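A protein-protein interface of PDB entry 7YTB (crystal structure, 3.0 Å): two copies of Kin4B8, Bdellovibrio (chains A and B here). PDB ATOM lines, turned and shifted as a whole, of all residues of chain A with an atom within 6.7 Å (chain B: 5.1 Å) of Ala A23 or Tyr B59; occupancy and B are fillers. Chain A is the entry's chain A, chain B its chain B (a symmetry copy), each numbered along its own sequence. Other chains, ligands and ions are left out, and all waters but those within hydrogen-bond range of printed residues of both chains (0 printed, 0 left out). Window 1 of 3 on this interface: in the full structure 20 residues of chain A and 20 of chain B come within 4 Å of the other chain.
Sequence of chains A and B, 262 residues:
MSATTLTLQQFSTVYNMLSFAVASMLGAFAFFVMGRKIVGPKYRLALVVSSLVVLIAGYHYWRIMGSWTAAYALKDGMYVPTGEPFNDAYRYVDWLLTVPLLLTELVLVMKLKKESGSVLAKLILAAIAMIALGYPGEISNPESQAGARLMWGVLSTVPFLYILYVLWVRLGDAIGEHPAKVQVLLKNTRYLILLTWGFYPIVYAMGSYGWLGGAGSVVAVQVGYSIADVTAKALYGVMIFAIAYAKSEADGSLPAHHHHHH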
ATOM      1  N   TYR A  15       8.331 -30.352 -28.607  1.00  0.00           N
ATOM      2  CA  TYR A  15       8.760 -29.720 -27.364  1.00  0.00           C
ATOM      3  C   TYR A  15      10.173 -30.146 -26.986  1.00  0.00           C
ATOM      4  O   TYR A  15      10.971 -29.329 -26.509  1.00  0.00           O
ATOM      5  CB  TYR A  15       7.781 -30.053 -26.238  1.00  0.00           C
ATOM      6  CG  TYR A  15       8.234 -29.571 -24.877  1.00  0.00           C
ATOM      7  CD1 TYR A  15       7.975 -28.276 -24.450  1.00  0.00           C
ATOM      8  CD2 TYR A  15       8.909 -30.420 -24.010  1.00  0.00           C
ATOM      9  CE1 TYR A  15       8.388 -27.834 -23.200  1.00  0.00           C
ATOM     10  CE2 TYR A  15       9.325 -29.990 -22.761  1.00  0.00           C
ATOM     11  CZ  TYR A  15       9.063 -28.697 -22.360  1.00  0.00           C
ATOM     12  OH  TYR A  15       9.474 -28.263 -21.117  1.00  0.00           O
ATOM     13  N   LEU A  18      12.761 -28.502 -29.116  1.00  0.00           N
ATOM     14  CA  LEU A  18      12.911 -27.125 -28.661  1.00  0.00           C
ATOM     15  C   LEU A  18      13.723 -27.054 -27.374  1.00  0.00           C
ATOM     16  O   LEU A  18      14.533 -26.138 -27.193  1.00  0.00           O
ATOM     17  CB  LEU A  18      11.537 -26.490 -28.469  1.00  0.00           C
ATOM     18  CG  LEU A  18      10.690 -26.321 -29.731  1.00  0.00           C
ATOM     19  CD1 LEU A  18       9.292 -25.835 -29.372  1.00  0.00           C
ATOM     20  CD2 LEU A  18      11.364 -25.373 -30.720  1.00  0.00           C
ATOM     21  N   SER A  19      13.516 -28.010 -26.465  1.00  0.00           N
ATOM     22  CA  SER A  19      14.316 -28.047 -25.245  1.00  0.00           C
ATOM     23  C   SER A  19      15.752 -28.464 -25.538  1.00  0.00           C
ATOM     24  O   SER A  19      16.686 -28.002 -24.873  1.00  0.00           O
ATOM     25  CB  SER A  19      13.680 -28.995 -24.225  1.00  0.00           C
ATOM     26  OG  SER A  19      13.076 -28.283 -23.158  1.00  0.00           O
ATOM     27  N   PHE A  20      15.945 -29.351 -26.520  1.00  0.00           N
ATOM     28  CA  PHE A  20      17.292 -29.664 -26.981  1.00  0.00           C
ATOM     29  C   PHE A  20      17.991 -28.412 -27.498  1.00  0.00           C
ATOM     30  O   PHE A  20      19.168 -28.178 -27.199  1.00  0.00           O
ATOM     31  CB  PHE A  20      17.244 -30.744 -28.063  1.00  0.00           C
ATOM     32  CG  PHE A  20      18.602 -31.169 -28.559  1.00  0.00           C
ATOM     33  CD1 PHE A  20      19.378 -32.040 -27.808  1.00  0.00           C
ATOM     34  CD2 PHE A  20      19.113 -30.691 -29.755  1.00  0.00           C
ATOM     35  CE1 PHE A  20      20.626 -32.439 -28.250  1.00  0.00           C
ATOM     36  CE2 PHE A  20      20.363 -31.085 -30.199  1.00  0.00           C
ATOM     37  CZ  PHE A  20      21.119 -31.959 -29.444  1.00  0.00           C
ATOM     38  N   ALA A  21      17.279 -27.600 -28.286  1.00  0.00           N
ATOM     39  CA  ALA A  21      17.875 -26.387 -28.841  1.00  0.00           C
ATOM     40  C   ALA A  21      18.260 -25.402 -27.744  1.00  0.00           C
ATOM     41  O   ALA A  21      19.342 -24.808 -27.790  1.00  0.00           O
ATOM     42  CB  ALA A  21      16.910 -25.737 -29.832  1.00  0.00           C
ATOM     43  N   VAL A  22      17.382 -25.202 -26.760  1.00  0.00           N
ATOM     44  CA  VAL A  22      17.690 -24.291 -25.658  1.00  0.00           C
ATOM     45  C   VAL A  22      18.956 -24.740 -24.936  1.00  0.00           C
ATOM     46  O   VAL A  22      19.856 -23.936 -24.663  1.00  0.00           O
ATOM     47  CB  VAL A  22      16.491 -24.186 -24.698  1.00  0.00           C
ATOM     48  CG1 VAL A  22      16.875 -23.401 -23.455  1.00  0.00           C
ATOM     49  CG2 VAL A  22      15.308 -23.535 -25.409  1.00  0.00           C
ATOM     50  N   ALA A  23      19.041 -26.034 -24.613  1.00  0.00           N
ATOM     51  CA  ALA A  23      20.199 -26.551 -23.889  1.00  0.00           C
ATOM     52  C   ALA A  23      21.474 -26.457 -24.724  1.00  0.00           C
ATOM     53  O   ALA A  23      22.550 -26.155 -24.191  1.00  0.00           O
ATOM     54  CB  ALA A  23      19.940 -27.991 -23.451  1.00  0.00           C
ATOM     55  N   SER A  24      21.377 -26.716 -26.031  1.00  0.00           N
ATOM     56  CA  SER A  24      22.556 -26.624 -26.888  1.00  0.00           C
ATOM     57  C   SER A  24      23.100 -25.199 -26.925  1.00  0.00           C
ATOM     58  O   SER A  24      24.316 -24.987 -26.871  1.00  0.00           O
ATOM     59  CB  SER A  24      22.220 -27.121 -28.296  1.00  0.00           C
ATOM     60  OG  SER A  24      21.762 -28.466 -28.271  1.00  0.00           O
ATOM     61  N   MET A  25      22.214 -24.207 -26.998  1.00  0.00           N
ATOM     62  CA  MET A  25      22.658 -22.816 -27.024  1.00  0.00           C
ATOM     63  C   MET A  25      23.278 -22.414 -25.692  1.00  0.00           C
ATOM     64  O   MET A  25      24.290 -21.704 -25.662  1.00  0.00           O
ATOM     65  CB  MET A  25      21.494 -21.895 -27.384  1.00  0.00           C
ATOM     66  CG  MET A  25      20.786 -22.288 -28.667  1.00  0.00           C
ATOM     67  SD  MET A  25      21.820 -22.130 -30.139  1.00  0.00           S
ATOM     68  CE  MET A  25      20.648 -22.553 -31.434  1.00  0.00           C
ATOM     69  N   LEU A  26      22.660 -22.823 -24.581  1.00  0.00           N
ATOM     70  CA  LEU A  26      23.204 -22.495 -23.267  1.00  0.00           C
ATOM     71  C   LEU A  26      24.581 -23.118 -23.080  1.00  0.00           C
ATOM     72  O   LEU A  26      25.489 -22.488 -22.523  1.00  0.00           O
ATOM     73  CB  LEU A  26      22.249 -22.968 -22.172  1.00  0.00           C
ATOM     74  CG  LEU A  26      22.738 -22.786 -20.736  1.00  0.00           C
ATOM     75  CD1 LEU A  26      22.983 -21.320 -20.445  1.00  0.00           C
ATOM     76  CD2 LEU A  26      21.745 -23.364 -19.746  1.00  0.00           C
ATOM     77  N   GLY A  27      24.749 -24.366 -23.522  1.00  0.00           N
ATOM     78  CA  GLY A  27      26.058 -24.989 -23.450  1.00  0.00           C
ATOM     79  C   GLY A  27      27.064 -24.311 -24.361  1.00  0.00           C
ATOM     80  O   GLY A  27      28.210 -24.074 -23.968  1.00  0.00           O
ATOM     81  N   ALA A  28      26.645 -23.967 -25.581  1.00  0.00           N
ATOM     82  CA  ALA A  28      27.550 -23.307 -26.517  1.00  0.00           C
ATOM     83  C   ALA A  28      27.950 -21.918 -26.032  1.00  0.00           C
ATOM     84  O   ALA A  28      29.096 -21.496 -26.227  1.00  0.00           O
ATOM     85  CB  ALA A  28      26.906 -23.226 -27.900  1.00  0.00           C
ATOM     86  N   TRP A  62      14.036 -20.183 -26.166  1.00  0.00           N
ATOM     87  CA  TRP A  62      13.304 -20.190 -24.904  1.00  0.00           C
ATOM     88  C   TRP A  62      11.901 -19.628 -25.091  1.00  0.00           C
ATOM     89  O   TRP A  62      10.928 -20.166 -24.547  1.00  0.00           O
ATOM     90  CB  TRP A  62      14.078 -19.386 -23.856  1.00  0.00           C
ATOM     91  CG  TRP A  62      13.365 -19.199 -22.549  1.00  0.00           C
ATOM     92  CD1 TRP A  62      12.778 -18.051 -22.100  1.00  0.00           C
ATOM     93  CD2 TRP A  62      13.168 -20.178 -21.520  1.00  0.00           C
ATOM     94  NE1 TRP A  62      12.229 -18.254 -20.858  1.00  0.00           N
ATOM     95  CE2 TRP A  62      12.453 -19.551 -20.480  1.00  0.00           C
ATOM     96  CE3 TRP A  62      13.526 -21.520 -21.377  1.00  0.00           C
ATOM     97  CZ2 TRP A  62      12.089 -20.222 -19.314  1.00  0.00           C
ATOM     98  CZ3 TRP A  62      13.161 -22.187 -20.219  1.00  0.00           C
ATOM     99  CH2 TRP A  62      12.451 -21.537 -19.203  1.00  0.00           C
ATOM    100  N   MET A  65       9.675 -22.012 -27.246  1.00  0.00           N
ATOM    101  CA  MET A  65       9.144 -23.097 -26.428  1.00  0.00           C
ATOM    102  C   MET A  65       7.911 -22.655 -25.650  1.00  0.00           C
ATOM    103  O   MET A  65       6.931 -23.402 -25.548  1.00  0.00           O
ATOM    104  CB  MET A  65      10.228 -23.595 -25.480  1.00  0.00           C
ATOM    105  CG  MET A  65       9.981 -24.955 -24.869  1.00  0.00           C
ATOM    106  SD  MET A  65      11.498 -25.448 -24.046  1.00  0.00           S
ATOM    107  CE  MET A  65      11.798 -23.944 -23.123  1.00  0.00           C
ATOM    108  N   VAL B  54      27.608 -30.391 -16.619  1.00  0.00           N
ATOM    109  CA  VAL B  54      26.796 -30.160 -15.430  1.00  0.00           C
ATOM    110  C   VAL B  54      25.872 -28.961 -15.615  1.00  0.00           C
ATOM    111  O   VAL B  54      24.788 -28.908 -15.018  1.00  0.00           O
ATOM    112  CB  VAL B  54      27.698 -30.009 -14.191  1.00  0.00           C
ATOM    113  CG1 VAL B  54      28.282 -31.354 -13.797  1.00  0.00           C
ATOM    114  CG2 VAL B  54      28.804 -29.006 -14.448  1.00  0.00           C
ATOM    115  N   LEU B  55      26.275 -27.983 -16.432  1.00  0.00           N
ATOM    116  CA  LEU B  55      25.397 -26.854 -16.720  1.00  0.00           C
ATOM    117  C   LEU B  55      24.152 -27.308 -17.468  1.00  0.00           C
ATOM    118  O   LEU B  55      23.028 -26.927 -17.119  1.00  0.00           O
ATOM    119  CB  LEU B  55      26.143 -25.801 -17.538  1.00  0.00           C
ATOM    120  CG  LEU B  55      25.303 -24.568 -17.889  1.00  0.00           C
ATOM    121  CD1 LEU B  55      24.950 -23.785 -16.638  1.00  0.00           C
ATOM    122  CD2 LEU B  55      26.011 -23.679 -18.895  1.00  0.00           C
ATOM    123  N   ILE B  56      24.339 -28.122 -18.507  1.00  0.00           N
ATOM    124  CA  ILE B  56      23.212 -28.626 -19.285  1.00  0.00           C
ATOM    125  C   ILE B  56      22.310 -29.490 -18.413  1.00  0.00           C
ATOM    126  O   ILE B  56      21.081 -29.340 -18.419  1.00  0.00           O
ATOM    127  CB  ILE B  56      23.721 -29.384 -20.521  1.00  0.00           C
ATOM    128  CG1 ILE B  56      24.543 -28.428 -21.386  1.00  0.00           C
ATOM    129  CG2 ILE B  56      22.563 -29.962 -21.315  1.00  0.00           C
ATOM    130  CD1 ILE B  56      25.137 -29.045 -22.609  1.00  0.00           C
ATOM    131  N   ALA B  57      22.906 -30.406 -17.645  1.00  0.00           N
ATOM    132  CA  ALA B  57      22.099 -31.257 -16.779  1.00  0.00           C
ATOM    133  C   ALA B  57      21.410 -30.438 -15.697  1.00  0.00           C
ATOM    134  O   ALA B  57      20.328 -30.812 -15.230  1.00  0.00           O
ATOM    135  CB  ALA B  57      22.960 -32.350 -16.153  1.00  0.00           C
ATOM    136  N   GLY B  58      22.027 -29.333 -15.278  1.00  0.00           N
ATOM    137  CA  GLY B  58      21.350 -28.424 -14.368  1.00  0.00           C
ATOM    138  C   GLY B  58      20.097 -27.841 -14.989  1.00  0.00           C
ATOM    139  O   GLY B  58      19.031 -27.819 -14.368  1.00  0.00           O
ATOM    140  N   TYR B  59      20.215 -27.342 -16.222  1.00  0.00           N
ATOM    141  CA  TYR B  59      19.050 -26.816 -16.924  1.00  0.00           C
ATOM    142  C   TYR B  59      17.980 -27.883 -17.122  1.00  0.00           C
ATOM    143  O   TYR B  59      16.787 -27.622 -16.928  1.00  0.00           O
ATOM    144  CB  TYR B  59      19.461 -26.245 -18.281  1.00  0.00           C
ATOM    145  CG  TYR B  59      18.282 -26.057 -19.207  1.00  0.00           C
ATOM    146  CD1 TYR B  59      17.393 -25.007 -19.027  1.00  0.00           C
ATOM    147  CD2 TYR B  59      18.045 -26.949 -20.246  1.00  0.00           C
ATOM    148  CE1 TYR B  59      16.305 -24.838 -19.870  1.00  0.00           C
ATOM    149  CE2 TYR B  59      16.959 -26.792 -21.094  1.00  0.00           C
ATOM    150  CZ  TYR B  59      16.092 -25.733 -20.900  1.00  0.00           C
ATOM    151  OH  TYR B  59      15.010 -25.567 -21.736  1.00  0.00           O
ATOM    152  N   HIS B  60      18.387 -29.090 -17.521  1.00  0.00           N
ATOM    153  CA  HIS B  60      17.411 -30.142 -17.786  1.00  0.00           C
ATOM    154  C   HIS B  60      16.721 -30.613 -16.513  1.00  0.00           C
ATOM    155  O   HIS B  60      15.517 -30.890 -16.525  1.00  0.00           O
ATOM    156  CB  HIS B  60      18.075 -31.304 -18.518  1.00  0.00           C
ATOM    157  CG  HIS B  60      18.219 -31.074 -19.989  1.00  0.00           C
ATOM    158  ND1 HIS B  60      17.160 -30.682 -20.778  1.00  0.00           N
ATOM    159  CD2 HIS B  60      19.285 -31.184 -20.815  1.00  0.00           C
ATOM    160  CE1 HIS B  60      17.567 -30.560 -22.029  1.00  0.00           C
ATOM    161  NE2 HIS B  60      18.852 -30.859 -22.079  1.00  0.00           N
ATOM    162  N   TYR B  61      17.461 -30.720 -15.410  1.00  0.00           N
ATOM    163  CA  TYR B  61      16.827 -31.109 -14.155  1.00  0.00           C
ATOM    164  C   TYR B  61      15.935 -30.007 -13.604  1.00  0.00           C
ATOM    165  O   TYR B  61      14.956 -30.297 -12.907  1.00  0.00           O
ATOM    166  CB  TYR B  61      17.880 -31.508 -13.128  1.00  0.00           C
ATOM    167  CG  TYR B  61      18.085 -32.999 -13.081  1.00  0.00           C
ATOM    168  CD1 TYR B  61      17.265 -33.799 -12.298  1.00  0.00           C
ATOM    169  CD2 TYR B  61      19.082 -33.610 -13.827  1.00  0.00           C
ATOM    170  CE1 TYR B  61      17.432 -35.168 -12.255  1.00  0.00           C
ATOM    171  CE2 TYR B  61      19.258 -34.979 -13.787  1.00  0.00           C
ATOM    172  CZ  TYR B  61      18.429 -35.754 -12.998  1.00  0.00           C
ATOM    173  OH  TYR B  61      18.595 -37.119 -12.952  1.00  0.00           O
ATOM    174  N   TRP B  62      16.267 -28.744 -13.881  1.00  0.00           N
ATOM    175  CA  TRP B  62      15.379 -27.651 -13.500  1.00  0.00           C
ATOM    176  C   TRP B  62      14.023 -27.791 -14.184  1.00  0.00           C
ATOM    177  O   TRP B  62      12.978 -27.540 -13.568  1.00  0.00           O
ATOM    178  CB  TRP B  62      16.030 -26.309 -13.837  1.00  0.00           C
ATOM    179  CG  TRP B  62      15.188 -25.116 -13.511  1.00  0.00           C
ATOM    180  CD1 TRP B  62      14.750 -24.745 -12.275  1.00  0.00           C
ATOM    181  CD2 TRP B  62      14.714 -24.114 -14.421  1.00  0.00           C
ATOM    182  NE1 TRP B  62      14.018 -23.588 -12.357  1.00  0.00           N
ATOM    183  CE2 TRP B  62      13.981 -23.177 -13.664  1.00  0.00           C
ATOM    184  CE3 TRP B  62      14.829 -23.919 -15.802  1.00  0.00           C
ATOM    185  CZ2 TRP B  62      13.366 -22.066 -14.239  1.00  0.00           C
ATOM    186  CZ3 TRP B  62      14.215 -22.812 -16.373  1.00  0.00           C
ATOM    187  CH2 TRP B  62      13.494 -21.901 -15.590  1.00  0.00           C
ATOM    188  N   ARG B  63      14.021 -28.177 -15.463  1.00  0.00           N
ATOM    189  CA  ARG B  63      12.763 -28.396 -16.170  1.00  0.00           C
ATOM    190  C   ARG B  63      12.045 -29.635 -15.646  1.00  0.00           C
ATOM    191  O   ARG B  63      10.816 -29.634 -15.511  1.00  0.00           O
ATOM    192  CB  ARG B  63      13.011 -28.532 -17.670  1.00  0.00           C
ATOM    193  CG  ARG B  63      13.789 -27.395 -18.292  1.00  0.00           C
ATOM    194  CD  ARG B  63      13.126 -26.047 -18.059  1.00  0.00           C
ATOM    195  NE  ARG B  63      11.702 -26.041 -18.368  1.00  0.00           N
ATOM    196  CZ  ARG B  63      11.196 -25.905 -19.584  1.00  0.00           C
ATOM    197  NH1 ARG B  63      11.977 -25.799 -20.643  1.00  0.00           N
ATOM    198  NH2 ARG B  63       9.876 -25.860 -19.738  1.00  0.00           N
ATOM    199  N   TYR B  90      12.102 -37.061 -21.682  1.00  0.00           N
ATOM    200  CA  TYR B  90      12.792 -35.780 -21.579  1.00  0.00           C
ATOM    201  C   TYR B  90      14.251 -35.976 -21.193  1.00  0.00           C
ATOM    202  O   TYR B  90      15.098 -35.132 -21.505  1.00  0.00           O
ATOM    203  CB  TYR B  90      12.109 -34.858 -20.576  1.00  0.00           C
ATOM    204  CG  TYR B  90      12.670 -33.459 -20.664  1.00  0.00           C
ATOM    205  CD1 TYR B  90      12.383 -32.639 -21.746  1.00  0.00           C
ATOM    206  CD2 TYR B  90      13.547 -32.987 -19.697  1.00  0.00           C
ATOM    207  CE1 TYR B  90      12.919 -31.370 -21.841  1.00  0.00           C
ATOM    208  CE2 TYR B  90      14.091 -31.720 -19.783  1.00  0.00           C
ATOM    209  CZ  TYR B  90      13.774 -30.915 -20.856  1.00  0.00           C
ATOM    210  OH  TYR B  90      14.314 -29.652 -20.942  1.00  0.00           O
ATOM    211  N   LEU B  97      22.977 -34.991 -25.629  1.00  0.00           N
ATOM    212  CA  LEU B  97      24.023 -33.981 -25.683  1.00  0.00           C
ATOM    213  C   LEU B  97      25.140 -34.275 -24.684  1.00  0.00           C
ATOM    214  O   LEU B  97      26.321 -34.155 -25.025  1.00  0.00           O
ATOM    215  CB  LEU B  97      23.404 -32.595 -25.448  1.00  0.00           C
ATOM    216  CG  LEU B  97      24.103 -31.304 -25.900  1.00  0.00           C
ATOM    217  CD1 LEU B  97      23.233 -30.110 -25.536  1.00  0.00           C
ATOM    218  CD2 LEU B  97      25.520 -31.111 -25.392  1.00  0.00           C
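The side-chain hydroxyl (OH) of Tyr A15 is in hydrogen-bond range of the guanidinium group (NH2) of Arg B63. The side-chain sulfur (SD) of Met A65 lies close to the guanidinium group (NH1) of Arg B63 (3.5 Å). The side-chain hydroxyl (OH) of Tyr B90 sits at hydrogen-bond distance from the side-chain hydroxyl (OG) of Ser A19 (2.9 Å).
The side-chain hydroxyl (OH) of Tyr B59 lies within hydrogen-bond range of the guanidinium group (NH1) of Arg B63 (3.2 Å). ND1 of His B60 lies within hydrogen-bond range of OH of Tyr B90, 3.0 Å away. O of Phe A20 sits at hydrogen-bond distance from OG of Ser A24, at 2.8 Å. The side-chain hydroxyl of Ser A19 sits at hydrogen-bond distance from the side-chain sulfur of Met A65, 3.4 Å away.
Among the printed residues, merely in contact across the chains: Tyr A15 with Tyr B90 (3.96 Å), Ser A19 with Tyr B59 (3.6 Å), Ser A19 with His B60 (3.9 Å), Ser A19 with Arg B63 (3.7 Å), Phe A20 with Leu B97 (3.9 Å), Val A22 with Tyr B59 (3.3 Å), Ala A23 with Ile B56 (3.9 Å), Ala A23 with Tyr B59 (3.9 Å), Ala A23 with His B60 (3.4 Å), Ser A24 with Leu B97 (3.5 Å), Leu A26 with Leu B55 (3.9 Å), Leu A26 with Tyr B59 (3.96 Å), Trp A62 with Trp B62 (3.6 Å), Trp A62 with Arg B63 (3.8 Å) and Met A65 with Tyr B59 (3.9 Å).
Printed residues of chain B within 4 Å of Tyr A15: Arg B63 (2.8 Å) and Tyr B90 (3.96 Å). Ala A23 touches just these residues of chain B: Ile B56 (3.9 Å), Tyr B59 (3.9 Å) and His B60 (3.4 Å). Of the printed residues of chain B, Ser A24 touches Leu B97. Of the printed residues of chain B, Leu A26 touches Leu B55 and Tyr B59. Of chain A, only Ser A19, Val A22, Ala A23, Leu A26 and Met A65 come within 4 Å of Tyr B59.
Of the 12 printed residues of chain B, 8 touch a printed residue of chain A. Hydrophobic or aromatic side chains of chain A within 4 Å of the printed part of chain B: Tyr A15, Phe A20, Val A22, Ala A23, Leu A26, Trp A62 and Met A65. Among the printed residues, 18 pairs touch across the chains.
Trp B62 touches its own counterpart, Trp A62. Position printed for both chains: 62.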
